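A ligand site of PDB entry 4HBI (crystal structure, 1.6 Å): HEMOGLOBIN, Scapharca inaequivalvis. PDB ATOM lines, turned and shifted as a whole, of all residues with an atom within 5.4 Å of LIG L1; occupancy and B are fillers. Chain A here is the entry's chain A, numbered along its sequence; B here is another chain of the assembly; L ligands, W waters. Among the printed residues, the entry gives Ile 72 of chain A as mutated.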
ATOM      1  N   LEU A  40      27.822  -7.027 -20.128  1.00  0.00           N
ATOM      2  CA  LEU A  40      27.268  -5.988 -20.992  1.00  0.00           C
ATOM      3  C   LEU A  40      28.403  -5.193 -21.618  1.00  0.00           C
ATOM      4  O   LEU A  40      28.440  -4.999 -22.831  1.00  0.00           O
ATOM      5  CB  LEU A  40      26.401  -5.027 -20.190  1.00  0.00           C
ATOM      6  CG  LEU A  40      25.805  -3.841 -20.935  1.00  0.00           C
ATOM      7  CD1 LEU A  40      24.708  -4.284 -21.880  1.00  0.00           C
ATOM      8  CD2 LEU A  40      25.267  -2.860 -19.926  1.00  0.00           C
ATOM      9  N   THR A  47      28.267   0.653 -25.041  1.00  0.00           N
ATOM     10  CA  THR A  47      27.444   1.129 -23.950  1.00  0.00           C
ATOM     11  C   THR A  47      28.258   1.766 -22.836  1.00  0.00           C
ATOM     12  O   THR A  47      27.716   2.545 -22.034  1.00  0.00           O
ATOM     13  CB  THR A  47      26.572  -0.018 -23.373  1.00  0.00           C
ATOM     14  OG1 THR A  47      27.448  -1.069 -22.944  1.00  0.00           O
ATOM     15  CG2 THR A  47      25.558  -0.506 -24.410  1.00  0.00           C
ATOM     16  N   TYR A  50      27.878   5.521 -21.730  1.00  0.00           N
ATOM     17  CA  TYR A  50      26.840   5.980 -20.798  1.00  0.00           C
ATOM     18  C   TYR A  50      27.293   5.946 -19.335  1.00  0.00           C
ATOM     19  O   TYR A  50      26.763   6.665 -18.480  1.00  0.00           O
ATOM     20  CB  TYR A  50      25.596   5.121 -20.942  1.00  0.00           C
ATOM     21  CG  TYR A  50      24.908   5.242 -22.296  1.00  0.00           C
ATOM     22  CD1 TYR A  50      24.205   6.406 -22.637  1.00  0.00           C
ATOM     23  CD2 TYR A  50      24.930   4.166 -23.170  1.00  0.00           C
ATOM     24  CE1 TYR A  50      23.514   6.486 -23.860  1.00  0.00           C
ATOM     25  CE2 TYR A  50      24.247   4.235 -24.388  1.00  0.00           C
ATOM     26  CZ  TYR A  50      23.548   5.390 -24.739  1.00  0.00           C
ATOM     27  OH  TYR A  50      22.885   5.436 -25.957  1.00  0.00           O
ATOM     28  N   PHE A  51      28.321   5.146 -19.047  1.00  0.00           N
ATOM     29  CA  PHE A  51      28.791   4.895 -17.704  1.00  0.00           C
ATOM     30  C   PHE A  51      30.121   5.539 -17.341  1.00  0.00           C
ATOM     31  O   PHE A  51      30.838   5.072 -16.456  1.00  0.00           O
ATOM     32  CB  PHE A  51      28.895   3.392 -17.509  1.00  0.00           C
ATOM     33  CG  PHE A  51      27.555   2.686 -17.598  1.00  0.00           C
ATOM     34  CD1 PHE A  51      26.799   2.505 -16.440  1.00  0.00           C
ATOM     35  CD2 PHE A  51      27.113   2.195 -18.825  1.00  0.00           C
ATOM     36  CE1 PHE A  51      25.585   1.826 -16.521  1.00  0.00           C
ATOM     37  CE2 PHE A  51      25.893   1.526 -18.896  1.00  0.00           C
ATOM     38  CZ  PHE A  51      25.129   1.337 -17.746  1.00  0.00           C
ATOM     39  N   ARG A  53      30.856   7.976 -15.468  1.00  0.00           N
ATOM     40  CA  ARG A  53      30.994   8.272 -14.047  1.00  0.00           C
ATOM     41  C   ARG A  53      31.545   7.099 -13.234  1.00  0.00           C
ATOM     42  O   ARG A  53      32.128   7.275 -12.155  1.00  0.00           O
ATOM     43  CB  ARG A  53      29.630   8.694 -13.470  1.00  0.00           C
ATOM     44  CG  ARG A  53      29.763   9.353 -12.095  1.00  0.00           C
ATOM     45  CD  ARG A  53      28.442   9.471 -11.352  1.00  0.00           C
ATOM     46  NE  ARG A  53      27.874   8.201 -10.885  1.00  0.00           N
ATOM     47  CZ  ARG A  53      28.348   7.526  -9.824  1.00  0.00           C
ATOM     48  NH1 ARG A  53      29.409   7.929  -9.120  1.00  0.00           N
ATOM     49  NH2 ARG A  53      27.676   6.457  -9.416  1.00  0.00           N
ATOM     50  N   LEU A  54      31.377   5.868 -13.714  1.00  0.00           N
ATOM     51  CA  LEU A  54      31.867   4.697 -13.007  1.00  0.00           C
ATOM     52  C   LEU A  54      33.382   4.524 -13.115  1.00  0.00           C
ATOM     53  O   LEU A  54      33.986   3.727 -12.392  1.00  0.00           O
ATOM     54  CB  LEU A  54      31.129   3.489 -13.556  1.00  0.00           C
ATOM     55  CG  LEU A  54      29.829   3.075 -12.868  1.00  0.00           C
ATOM     56  CD1 LEU A  54      28.943   4.263 -12.533  1.00  0.00           C
ATOM     57  CD2 LEU A  54      29.110   2.138 -13.802  1.00  0.00           C
ATOM     58  N   HIS A  69      26.935   0.355  -8.216  1.00  0.00           N
ATOM     59  CA  HIS A  69      25.898   0.355  -9.239  1.00  0.00           C
ATOM     60  C   HIS A  69      25.306  -1.044  -9.436  1.00  0.00           C
ATOM     61  O   HIS A  69      24.081  -1.209  -9.480  1.00  0.00           O
ATOM     62  CB  HIS A  69      26.461   0.875 -10.572  1.00  0.00           C
ATOM     63  CG  HIS A  69      25.477   0.741 -11.742  1.00  0.00           C
ATOM     64  ND1 HIS A  69      24.408   1.502 -11.828  1.00  0.00           N
ATOM     65  CD2 HIS A  69      25.498  -0.239 -12.709  1.00  0.00           C
ATOM     66  CE1 HIS A  69      23.741   1.000 -12.848  1.00  0.00           C
ATOM     67  NE2 HIS A  69      24.392  -0.016 -13.365  1.00  0.00           N
ATOM     68  N   ILE A  72      22.931  -2.136  -6.611  1.00  0.00           N
ATOM     69  CA  ILE A  72      21.692  -1.371  -6.684  1.00  0.00           C
ATOM     70  C   ILE A  72      20.837  -1.843  -7.852  1.00  0.00           C
ATOM     71  O   ILE A  72      19.615  -1.939  -7.688  1.00  0.00           O
ATOM     72  CB  ILE A  72      22.070   0.156  -6.796  1.00  0.00           C
ATOM     73  CG1 ILE A  72      22.617   0.574  -5.423  1.00  0.00           C
ATOM     74  CG2 ILE A  72      20.880   1.022  -7.222  1.00  0.00           C
ATOM     75  CD1 ILE A  72      22.676   2.077  -5.062  1.00  0.00           C
ATOM     76  N   LEU A  73      21.445  -2.178  -9.002  1.00  0.00           N
ATOM     77  CA  LEU A  73      20.704  -2.704 -10.152  1.00  0.00           C
ATOM     78  C   LEU A  73      19.912  -3.954  -9.749  1.00  0.00           C
ATOM     79  O   LEU A  73      18.727  -4.097 -10.086  1.00  0.00           O
ATOM     80  CB  LEU A  73      21.695  -3.025 -11.293  1.00  0.00           C
ATOM     81  CG  LEU A  73      21.187  -3.627 -12.616  1.00  0.00           C
ATOM     82  CD1 LEU A  73      22.073  -3.179 -13.741  1.00  0.00           C
ATOM     83  CD2 LEU A  73      21.195  -5.161 -12.557  1.00  0.00           C
ATOM     84  N   ALA A  76      16.592  -3.333  -8.042  1.00  0.00           N
ATOM     85  CA  ALA A  76      15.530  -2.922  -8.949  1.00  0.00           C
ATOM     86  C   ALA A  76      14.891  -4.186  -9.529  1.00  0.00           C
ATOM     87  O   ALA A  76      13.670  -4.287  -9.665  1.00  0.00           O
ATOM     88  CB  ALA A  76      16.071  -2.081 -10.108  1.00  0.00           C
ATOM     89  N   LEU A  77      15.692  -5.212  -9.876  1.00  0.00           N
ATOM     90  CA  LEU A  77      15.158  -6.505 -10.332  1.00  0.00           C
ATOM     91  C   LEU A  77      14.348  -7.182  -9.220  1.00  0.00           C
ATOM     92  O   LEU A  77      13.230  -7.653  -9.448  1.00  0.00           O
ATOM     93  CB  LEU A  77      16.322  -7.357 -10.769  1.00  0.00           C
ATOM     94  CG  LEU A  77      16.609  -7.611 -12.248  1.00  0.00           C
ATOM     95  CD1 LEU A  77      16.052  -6.527 -13.148  1.00  0.00           C
ATOM     96  CD2 LEU A  77      18.098  -7.790 -12.376  1.00  0.00           C
ATOM     97  N   PHE A  80      10.958  -5.526  -9.104  1.00  0.00           N
ATOM     98  CA  PHE A  80      10.069  -6.000 -10.173  1.00  0.00           C
ATOM     99  C   PHE A  80       9.500  -7.373  -9.890  1.00  0.00           C
ATOM    100  O   PHE A  80       8.299  -7.586 -10.033  1.00  0.00           O
ATOM    101  CB  PHE A  80      10.817  -6.045 -11.506  1.00  0.00           C
ATOM    102  CG  PHE A  80      11.335  -4.710 -12.041  1.00  0.00           C
ATOM    103  CD1 PHE A  80      10.796  -3.485 -11.621  1.00  0.00           C
ATOM    104  CD2 PHE A  80      12.372  -4.720 -12.984  1.00  0.00           C
ATOM    105  CE1 PHE A  80      11.303  -2.285 -12.127  1.00  0.00           C
ATOM    106  CE2 PHE A  80      12.865  -3.519 -13.487  1.00  0.00           C
ATOM    107  CZ  PHE A  80      12.328  -2.297 -13.054  1.00  0.00           C
ATOM    108  N   PHE A  97      10.919   3.943 -12.488  1.00  0.00           N
ATOM    109  CA  PHE A  97      12.263   3.507 -12.832  1.00  0.00           C
ATOM    110  C   PHE A  97      12.719   4.070 -14.178  1.00  0.00           C
ATOM    111  O   PHE A  97      13.889   4.414 -14.407  1.00  0.00           O
ATOM    112  CB  PHE A  97      12.240   1.985 -12.832  1.00  0.00           C
ATOM    113  CG  PHE A  97      13.413   1.289 -13.499  1.00  0.00           C
ATOM    114  CD1 PHE A  97      13.369   0.999 -14.876  1.00  0.00           C
ATOM    115  CD2 PHE A  97      14.535   0.957 -12.740  1.00  0.00           C
ATOM    116  CE1 PHE A  97      14.450   0.383 -15.478  1.00  0.00           C
ATOM    117  CE2 PHE A  97      15.605   0.335 -13.364  1.00  0.00           C
ATOM    118  CZ  PHE A  97      15.570   0.053 -14.733  1.00  0.00           C
ATOM    119  N   ASN A 100      14.608   8.184 -14.968  1.00  0.00           N
ATOM    120  CA  ASN A 100      16.022   8.491 -15.096  1.00  0.00           C
ATOM    121  C   ASN A 100      16.661   7.916 -16.356  1.00  0.00           C
ATOM    122  O   ASN A 100      17.587   8.515 -16.904  1.00  0.00           O
ATOM    123  CB  ASN A 100      16.769   7.980 -13.882  1.00  0.00           C
ATOM    124  CG  ASN A 100      16.492   8.752 -12.600  1.00  0.00           C
ATOM    125  OD1 ASN A 100      15.823   9.787 -12.591  1.00  0.00           O
ATOM    126  ND2 ASN A 100      16.964   8.288 -11.459  1.00  0.00           N
ATOM    127  N   HIS A 101      16.164   6.791 -16.869  1.00  0.00           N
ATOM    128  CA  HIS A 101      16.715   6.197 -18.084  1.00  0.00           C
ATOM    129  C   HIS A 101      16.287   7.032 -19.284  1.00  0.00           C
ATOM    130  O   HIS A 101      17.090   7.233 -20.207  1.00  0.00           O
ATOM    131  CB  HIS A 101      16.246   4.735 -18.208  1.00  0.00           C
ATOM    132  CG  HIS A 101      16.904   3.831 -17.156  1.00  0.00           C
ATOM    133  ND1 HIS A 101      16.428   3.623 -15.857  1.00  0.00           N
ATOM    134  CD2 HIS A 101      18.118   3.151 -17.355  1.00  0.00           C
ATOM    135  CE1 HIS A 101      17.368   2.848 -15.283  1.00  0.00           C
ATOM    136  NE2 HIS A 101      18.339   2.542 -16.114  1.00  0.00           N
ATOM    137  N   ARG A 104      18.482  10.086 -19.444  1.00  0.00           N
ATOM    138  CA  ARG A 104      19.787   9.750 -20.020  1.00  0.00           C
ATOM    139  C   ARG A 104      19.748   9.341 -21.490  1.00  0.00           C
ATOM    140  O   ARG A 104      20.788   8.977 -22.051  1.00  0.00           O
ATOM    141  CB  ARG A 104      20.418   8.609 -19.257  1.00  0.00           C
ATOM    142  CG  ARG A 104      20.778   8.980 -17.864  1.00  0.00           C
ATOM    143  CD  ARG A 104      21.164   7.715 -17.143  1.00  0.00           C
ATOM    144  NE  ARG A 104      21.295   8.098 -15.757  1.00  0.00           N
ATOM    145  CZ  ARG A 104      20.627   7.498 -14.770  1.00  0.00           C
ATOM    146  NH1 ARG A 104      19.787   6.456 -14.956  1.00  0.00           N
ATOM    147  NH2 ARG A 104      20.788   8.040 -13.572  1.00  0.00           N
ATOM    148  N   ILE A 106      18.332   6.660 -22.952  1.00  0.00           N
ATOM    149  CA  ILE A 106      18.530   5.231 -23.093  1.00  0.00           C
ATOM    150  C   ILE A 106      17.243   4.831 -23.812  1.00  0.00           C
ATOM    151  O   ILE A 106      16.153   4.965 -23.246  1.00  0.00           O
ATOM    152  CB  ILE A 106      18.604   4.483 -21.722  1.00  0.00           C
ATOM    153  CG1 ILE A 106      19.648   5.050 -20.756  1.00  0.00           C
ATOM    154  CG2 ILE A 106      18.931   3.038 -22.031  1.00  0.00           C
ATOM    155  CD1 ILE A 106      21.100   5.083 -21.240  1.00  0.00           C
ATOM    156  N   GLU A 110      18.387   0.297 -26.776  1.00  0.00           N
ATOM    157  CA  GLU A 110      19.591   0.336 -25.974  1.00  0.00           C
ATOM    158  C   GLU A 110      19.385  -0.528 -24.733  1.00  0.00           C
ATOM    159  O   GLU A 110      20.234  -1.350 -24.392  1.00  0.00           O
ATOM    160  CB  GLU A 110      19.846   1.775 -25.575  1.00  0.00           C
ATOM    161  CG  GLU A 110      21.290   2.113 -25.267  1.00  0.00           C
ATOM    162  CD  GLU A 110      22.167   2.254 -26.501  1.00  0.00           C
ATOM    163  OE1 GLU A 110      21.900   3.120 -27.344  1.00  0.00           O
ATOM    164  OE2 GLU A 110      23.149   1.508 -26.603  1.00  0.00           O
ATOM    165  N   PHE A 111      18.235  -0.374 -24.060  1.00  0.00           N
ATOM    166  CA  PHE A 111      17.904  -1.137 -22.876  1.00  0.00           C
ATOM    167  C   PHE A 111      17.876  -2.642 -23.177  1.00  0.00           C
ATOM    168  O   PHE A 111      18.393  -3.459 -22.408  1.00  0.00           O
ATOM    169  CB  PHE A 111      16.550  -0.689 -22.340  1.00  0.00           C
ATOM    170  CG  PHE A 111      16.338  -1.041 -20.859  1.00  0.00           C
ATOM    171  CD1 PHE A 111      16.803  -0.170 -19.869  1.00  0.00           C
ATOM    172  CD2 PHE A 111      15.735  -2.250 -20.499  1.00  0.00           C
ATOM    173  CE1 PHE A 111      16.670  -0.508 -18.528  1.00  0.00           C
ATOM    174  CE2 PHE A 111      15.596  -2.588 -19.150  1.00  0.00           C
ATOM    175  CZ  PHE A 111      16.058  -1.715 -18.174  1.00  0.00           C
ATOM    176  N   ILE A 114      20.575  -5.529 -22.539  1.00  0.00           N
ATOM    177  CA  ILE A 114      20.763  -6.276 -21.309  1.00  0.00           C
ATOM    178  C   ILE A 114      20.324  -7.732 -21.423  1.00  0.00           C
ATOM    179  O   ILE A 114      20.756  -8.585 -20.632  1.00  0.00           O
ATOM    180  CB  ILE A 114      20.000  -5.560 -20.165  1.00  0.00           C
ATOM    181  CG1 ILE A 114      20.660  -5.985 -18.858  1.00  0.00           C
ATOM    182  CG2 ILE A 114      18.488  -5.863 -20.196  1.00  0.00           C
ATOM    183  CD1 ILE A 114      22.145  -5.529 -18.747  1.00  0.00           C
ATOM    184  N   ILE A 118      21.803 -11.126 -19.473  1.00  0.00           N
ATOM    185  CA  ILE A 118      20.909 -11.934 -18.646  1.00  0.00           C
ATOM    186  C   ILE A 118      20.922 -13.388 -19.112  1.00  0.00           C
ATOM    187  O   ILE A 118      21.101 -14.276 -18.274  1.00  0.00           O
ATOM    188  CB  ILE A 118      19.448 -11.369 -18.676  1.00  0.00           C
ATOM    189  CG1 ILE A 118      19.419 -10.036 -17.946  1.00  0.00           C
ATOM    190  CG2 ILE A 118      18.471 -12.321 -17.984  1.00  0.00           C
ATOM    191  CD1 ILE A 118      18.060  -9.311 -17.950  1.00  0.00           C
ATOM    192  N   VAL A 139      11.895  -7.538 -19.305  1.00  0.00           N
ATOM    193  CA  VAL A 139      12.647  -6.414 -19.861  1.00  0.00           C
ATOM    194  C   VAL A 139      11.791  -5.684 -20.912  1.00  0.00           C
ATOM    195  O   VAL A 139      11.853  -4.452 -21.033  1.00  0.00           O
ATOM    196  CB  VAL A 139      13.968  -6.947 -20.479  1.00  0.00           C
ATOM    197  CG1 VAL A 139      14.725  -5.872 -21.247  1.00  0.00           C
ATOM    198  CG2 VAL A 139      14.875  -7.408 -19.354  1.00  0.00           C
ATOM    199  N   LYS B  96      26.874   5.731  -4.245  1.00  0.00           N
ATOM    200  CA  LYS B  96      26.177   5.637  -5.525  1.00  0.00           C
ATOM    201  C   LYS B  96      24.778   6.235  -5.406  1.00  0.00           C
ATOM    202  O   LYS B  96      24.364   7.032  -6.238  1.00  0.00           O
ATOM    203  CB  LYS B  96      26.109   4.165  -5.952  1.00  0.00           C
ATOM    204  CG  LYS B  96      25.088   3.743  -7.013  1.00  0.00           C
ATOM    205  CD  LYS B  96      25.230   4.284  -8.430  1.00  0.00           C
ATOM    206  CE  LYS B  96      24.022   3.739  -9.179  1.00  0.00           C
ATOM    207  NZ  LYS B  96      23.997   4.158 -10.555  1.00  0.00           N
ATOM    208  N   ASN B 100      22.417  11.031  -7.347  1.00  0.00           N
ATOM    209  CA  ASN B 100      21.216  11.697  -7.849  1.00  0.00           C
ATOM    210  C   ASN B 100      20.609  12.677  -6.865  1.00  0.00           C
ATOM    211  O   ASN B 100      20.058  13.695  -7.269  1.00  0.00           O
ATOM    212  CB  ASN B 100      20.120  10.685  -8.208  1.00  0.00           C
ATOM    213  CG  ASN B 100      20.368   9.851  -9.467  1.00  0.00           C
ATOM    214  OD1 ASN B 100      21.271  10.086 -10.276  1.00  0.00           O
ATOM    215  ND2 ASN B 100      19.564   8.827  -9.662  1.00  0.00           N
HETATM  216  C1  LIG L   1      21.410   3.608 -13.277  1.00  0.00           C
HETATM  217  C2  LIG L   1      18.801  -0.354 -13.040  1.00  0.00           C
HETATM  218  C3  LIG L   1      19.875  -1.321 -17.610  1.00  0.00           C
HETATM  219  C4  LIG L   1      22.105   2.881 -17.980  1.00  0.00           C
HETATM  220  C5  LIG L   1      20.494   2.679 -12.837  1.00  0.00           C
HETATM  221  C6  LIG L   1      20.001   2.583 -11.465  1.00  0.00           C
HETATM  222  C7  LIG L   1      19.253   1.466 -11.416  1.00  0.00           C
HETATM  223  C8  LIG L   1      19.298   0.884 -12.740  1.00  0.00           C
HETATM  224  C9  LIG L   1      18.454   0.968 -10.218  1.00  0.00           C
HETATM  225  C10 LIG L   1      20.177   3.578 -10.316  1.00  0.00           C
HETATM  226  C11 LIG L   1      19.043   4.622 -10.213  1.00  0.00           C
HETATM  227  C12 LIG L   1      19.010   5.609 -11.383  1.00  0.00           C
HETATM  228  O1  LIG L   1      19.854   6.475 -11.445  1.00  0.00           O
HETATM  229  O2  LIG L   1      18.143   5.518 -12.252  1.00  0.00           O
HETATM  230  C13 LIG L   1      18.867  -0.974 -14.264  1.00  0.00           C
HETATM  231  C14 LIG L   1      18.335  -2.297 -14.523  1.00  0.00           C
HETATM  232  C15 LIG L   1      18.656  -2.583 -15.817  1.00  0.00           C
HETATM  233  C16 LIG L   1      19.361  -1.421 -16.330  1.00  0.00           C
HETATM  234  C17 LIG L   1      17.504  -3.107 -13.524  1.00  0.00           C
HETATM  235  C18 LIG L   1      18.333  -3.704 -16.588  1.00  0.00           C
HETATM  236  C19 LIG L   1      18.222  -5.074 -16.142  1.00  0.00           C
HETATM  237  C20 LIG L   1      20.537  -0.233 -18.136  1.00  0.00           C
HETATM  238  C21 LIG L   1      21.090  -0.189 -19.468  1.00  0.00           C
HETATM  239  C22 LIG L   1      21.695   1.035 -19.600  1.00  0.00           C
HETATM  240  C23 LIG L   1      21.496   1.689 -18.321  1.00  0.00           C
HETATM  241  C24 LIG L   1      20.992  -1.335 -20.473  1.00  0.00           C
HETATM  242  C25 LIG L   1      22.380   1.635 -20.662  1.00  0.00           C
HETATM  243  C26 LIG L   1      22.948   1.025 -21.853  1.00  0.00           C
HETATM  244  C27 LIG L   1      22.134   3.434 -16.716  1.00  0.00           C
HETATM  245  C28 LIG L   1      23.035   4.491 -16.335  1.00  0.00           C
HETATM  246  C29 LIG L   1      22.905   4.642 -14.999  1.00  0.00           C
HETATM  247  C30 LIG L   1      21.893   3.693 -14.569  1.00  0.00           C
HETATM  248  C31 LIG L   1      23.946   5.284 -17.275  1.00  0.00           C
HETATM  249  C32 LIG L   1      23.689   5.579 -14.104  1.00  0.00           C
HETATM  250  C33 LIG L   1      25.045   5.038 -13.714  1.00  0.00           C
HETATM  251  C34 LIG L   1      25.829   6.037 -12.889  1.00  0.00           C
HETATM  252  O3  LIG L   1      26.351   6.993 -13.467  1.00  0.00           O
HETATM  253  O4  LIG L   1      25.908   5.863 -11.676  1.00  0.00           O
HETATM  254  N1  LIG L   1      19.995   1.669 -13.628  1.00  0.00           N
HETATM  255  N2  LIG L   1      19.452  -0.416 -15.391  1.00  0.00           N
HETATM  256  N3  LIG L   1      20.773   0.926 -17.425  1.00  0.00           N
HETATM  257  N4  LIG L   1      21.446   2.922 -15.625  1.00  0.00           N
HETATM  258 FE1  LIG L   1      20.195   1.417 -15.593  1.00  0.00          FE
HETATM  259  C1  LG2 L   2      14.383   9.663  -5.684  1.00  0.00           C
HETATM  260  C2  LG2 L   2      15.405   6.941  -1.898  1.00  0.00           C
HETATM  261  C3  LG2 L   2      14.876  10.734   0.956  1.00  0.00           C
HETATM  262  C4  LG2 L   2      14.095  13.516  -2.835  1.00  0.00           C
HETATM  263  C5  LG2 L   2      14.818   8.601  -4.922  1.00  0.00           C
HETATM  264  C6  LG2 L   2      15.030   7.254  -5.406  1.00  0.00           C
HETATM  265  C7  LG2 L   2      15.327   6.492  -4.333  1.00  0.00           C
HETATM  266  C8  LG2 L   2      15.285   7.365  -3.193  1.00  0.00           C
HETATM  267  C9  LG2 L   2      15.713   5.020  -4.314  1.00  0.00           C
HETATM  268  C10 LG2 L   2      14.962   6.783  -6.853  1.00  0.00           C
HETATM  269  C11 LG2 L   2      16.312   6.854  -7.584  1.00  0.00           C
HETATM  270  C12 LG2 L   2      16.800   8.276  -7.810  1.00  0.00           C
HETATM  271  O1  LG2 L   2      16.250   8.939  -8.680  1.00  0.00           O
HETATM  272  O2  LG2 L   2      17.698   8.738  -7.122  1.00  0.00           O
HETATM  273  C13 LG2 L   2      15.373   7.738  -0.794  1.00  0.00           C
HETATM  274  C14 LG2 L   2      15.539   7.239   0.554  1.00  0.00           C
HETATM  275  C15 LG2 L   2      15.366   8.316   1.379  1.00  0.00           C
HETATM  276  C16 LG2 L   2      15.140   9.458   0.504  1.00  0.00           C
HETATM  277  C17 LG2 L   2      15.973   5.831   0.925  1.00  0.00           C
HETATM  278  C18 LG2 L   2      15.449   8.409   2.767  1.00  0.00           C
HETATM  279  C19 LG2 L   2      15.020   7.433   3.748  1.00  0.00           C
HETATM  280  C20 LG2 L   2      14.677  11.839   0.172  1.00  0.00           C
HETATM  281  C21 LG2 L   2      14.378  13.156   0.701  1.00  0.00           C
HETATM  282  C22 LG2 L   2      14.212  13.979  -0.382  1.00  0.00           C
HETATM  283  C23 LG2 L   2      14.373  13.118  -1.545  1.00  0.00           C
HETATM  284  C24 LG2 L   2      14.313  13.480   2.187  1.00  0.00           C
HETATM  285  C25 LG2 L   2      14.011  15.361  -0.459  1.00  0.00           C
HETATM  286  C26 LG2 L   2      13.270  16.201   0.464  1.00  0.00           C
HETATM  287  C27 LG2 L   2      14.109  12.712  -3.952  1.00  0.00           C
HETATM  288  C28 LG2 L   2      13.589  13.121  -5.232  1.00  0.00           C
HETATM  289  C29 LG2 L   2      13.611  12.020  -6.009  1.00  0.00           C
HETATM  290  C30 LG2 L   2      14.178  10.952  -5.225  1.00  0.00           C
HETATM  291  C31 LG2 L   2      13.070  14.515  -5.592  1.00  0.00           C
HETATM  292  C32 LG2 L   2      13.001  11.873  -7.391  1.00  0.00           C
HETATM  293  C33 LG2 L   2      11.501  11.695  -7.316  1.00  0.00           C
HETATM  294  C34 LG2 L   2      10.843  11.631  -8.676  1.00  0.00           C
HETATM  295  O3  LG2 L   2      10.385  12.664  -9.172  1.00  0.00           O
HETATM  296  O4  LG2 L   2      10.819  10.555  -9.260  1.00  0.00           O
HETATM  297  N1  LG2 L   2      15.045   8.675  -3.566  1.00  0.00           N
HETATM  298  N2  LG2 L   2      15.201   9.110  -0.826  1.00  0.00           N
HETATM  299  N3  LG2 L   2      14.708  11.827  -1.213  1.00  0.00           N
HETATM  300  N4  LG2 L   2      14.452  11.368  -3.942  1.00  0.00           N
HETATM  301 FE1  LG2 L   2      15.103  10.291  -2.424  1.00  0.00          FE
HETATM  302  O   HOH W   1      15.611   4.423 -12.007  1.00  0.00           O
HETATM  303  O   HOH W   2      25.405   9.795 -13.147  1.00  0.00           O
HETATM  304  O   HOH W   3      21.518   4.980  -7.565  1.00  0.00           O
HETATM  305  O   HOH W   4      22.392   6.447 -10.017  1.00  0.00           O
HETATM  306  O   HOH W   5      27.919   7.542 -16.036  1.00  0.00           O
HETATM  307  O   HOH W   6      23.022  -0.705 -15.840  1.00  0.00           O
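An iron atom (FE1) of LIG L1 is bound by a ring nitrogen (NE2) of His 101.
The side-chain amino group (NZ) of Lys 96 of chain B is in salt-bridge range of an oxygen (O4) of LIG L1 (2.8 Å).
NH2 of Arg 104 lies within salt-bridge range of O1 of LIG L1 (2.8 Å).
An oxygen (O4) of LIG L1 is in salt-bridge range of the guanidinium group (NH2) of Arg 53 (2.9 Å).
An oxygen (O1) of LIG L1 lies within hydrogen-bond range of the side-chain amide nitrogen (ND2) of Asn 100 of chain B (3.0 Å).
An oxygen (O2) of LIG L1 is in hydrogen-bond range of the side-chain amide nitrogen (ND2) of Asn 100 of chain A (3.1 Å).
ND2 of Asn 100 of chain B sits at hydrogen-bond distance from O2 of LG2 L2, 3.2 Å away.
ND2 of Asn 100 of chain A is in hydrogen-bond range of O1 of LG2 L2, at 2.9 Å.
A ring nitrogen (ND1) of His 101 is in hydrogen-bond range of the backbone carbonyl oxygen of Phe 97 (3.0 Å).
O of His 101 lies within hydrogen-bond range of N of Ile 106, 3.1 Å away.
The side-chain amino group (NZ) of Lys 96 of chain B sits at hydrogen-bond distance from a ring nitrogen (ND1) of His 69 (3.0 Å).
ND2 of Asn 100 of chain B lies close to ND2 of Asn 100 of chain A.
The side-chain carboxylate (OE1) of Glu 110 sits at hydrogen-bond distance from the side-chain hydroxyl (OH) of Tyr 50.
Thr 47 touches LIG L1.
Tyr 50 touches LIG L1 (O to C31, 3.4 Å).
Phe 51 touches LIG L1 (CZ to C4, 3.4 Å).
CD1 of Leu 54 touches O4 of LIG L1, at 3.5 Å.
His 69 touches LIG L1 (CE1 to C1, 3.5 Å).
Ile 72 touches LIG L1 (CG2 to C9, 3.9 Å).
Leu 73 touches LIG L1.
Ala 76 touches LIG L1.
CD1 of Leu 77 touches C17 of LIG L1 (3.7 Å).
Phe 97 touches LIG L1 (CE2 to C2, 3.3 Å).
CD1 of Ile 106 touches C25 of LIG L1, 3.7 Å away.
CG of Glu 110 touches C26 of LIG L1 (3.9 Å).
Phe 111 touches LIG L1.
Ile 114 touches LIG L1 (CG1 to C19, 3.8 Å).
Hydrophobic or aromatic side chains that line LIG L1: Tyr 50, Phe 51, Leu 54, His 69, Ile 72, Leu 73, Ala 76, Leu 77, Phe 97, His 101, Ile 106, Phe 111 and Ile 114.
Of the 24 residues printed, 20 come within 4 Å of LIG L1.
The nearest printed residue that does not touch LIG L1 is Leu 40 (4.6 Å).
Water W1 lies within hydrogen-bond range of an oxygen (O2) of LIG L1 (2.8 Å) and the backbone carbonyl oxygen (O) of Phe 97 (3.0 Å).
Water W4 lies within hydrogen-bond range of the side-chain amino group of Lys 96 of chain B and an oxygen (O1) of LIG L1.
Water W5 lies within hydrogen-bond range of O of Tyr 50, N of Arg 53 and O3 of LIG L1.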
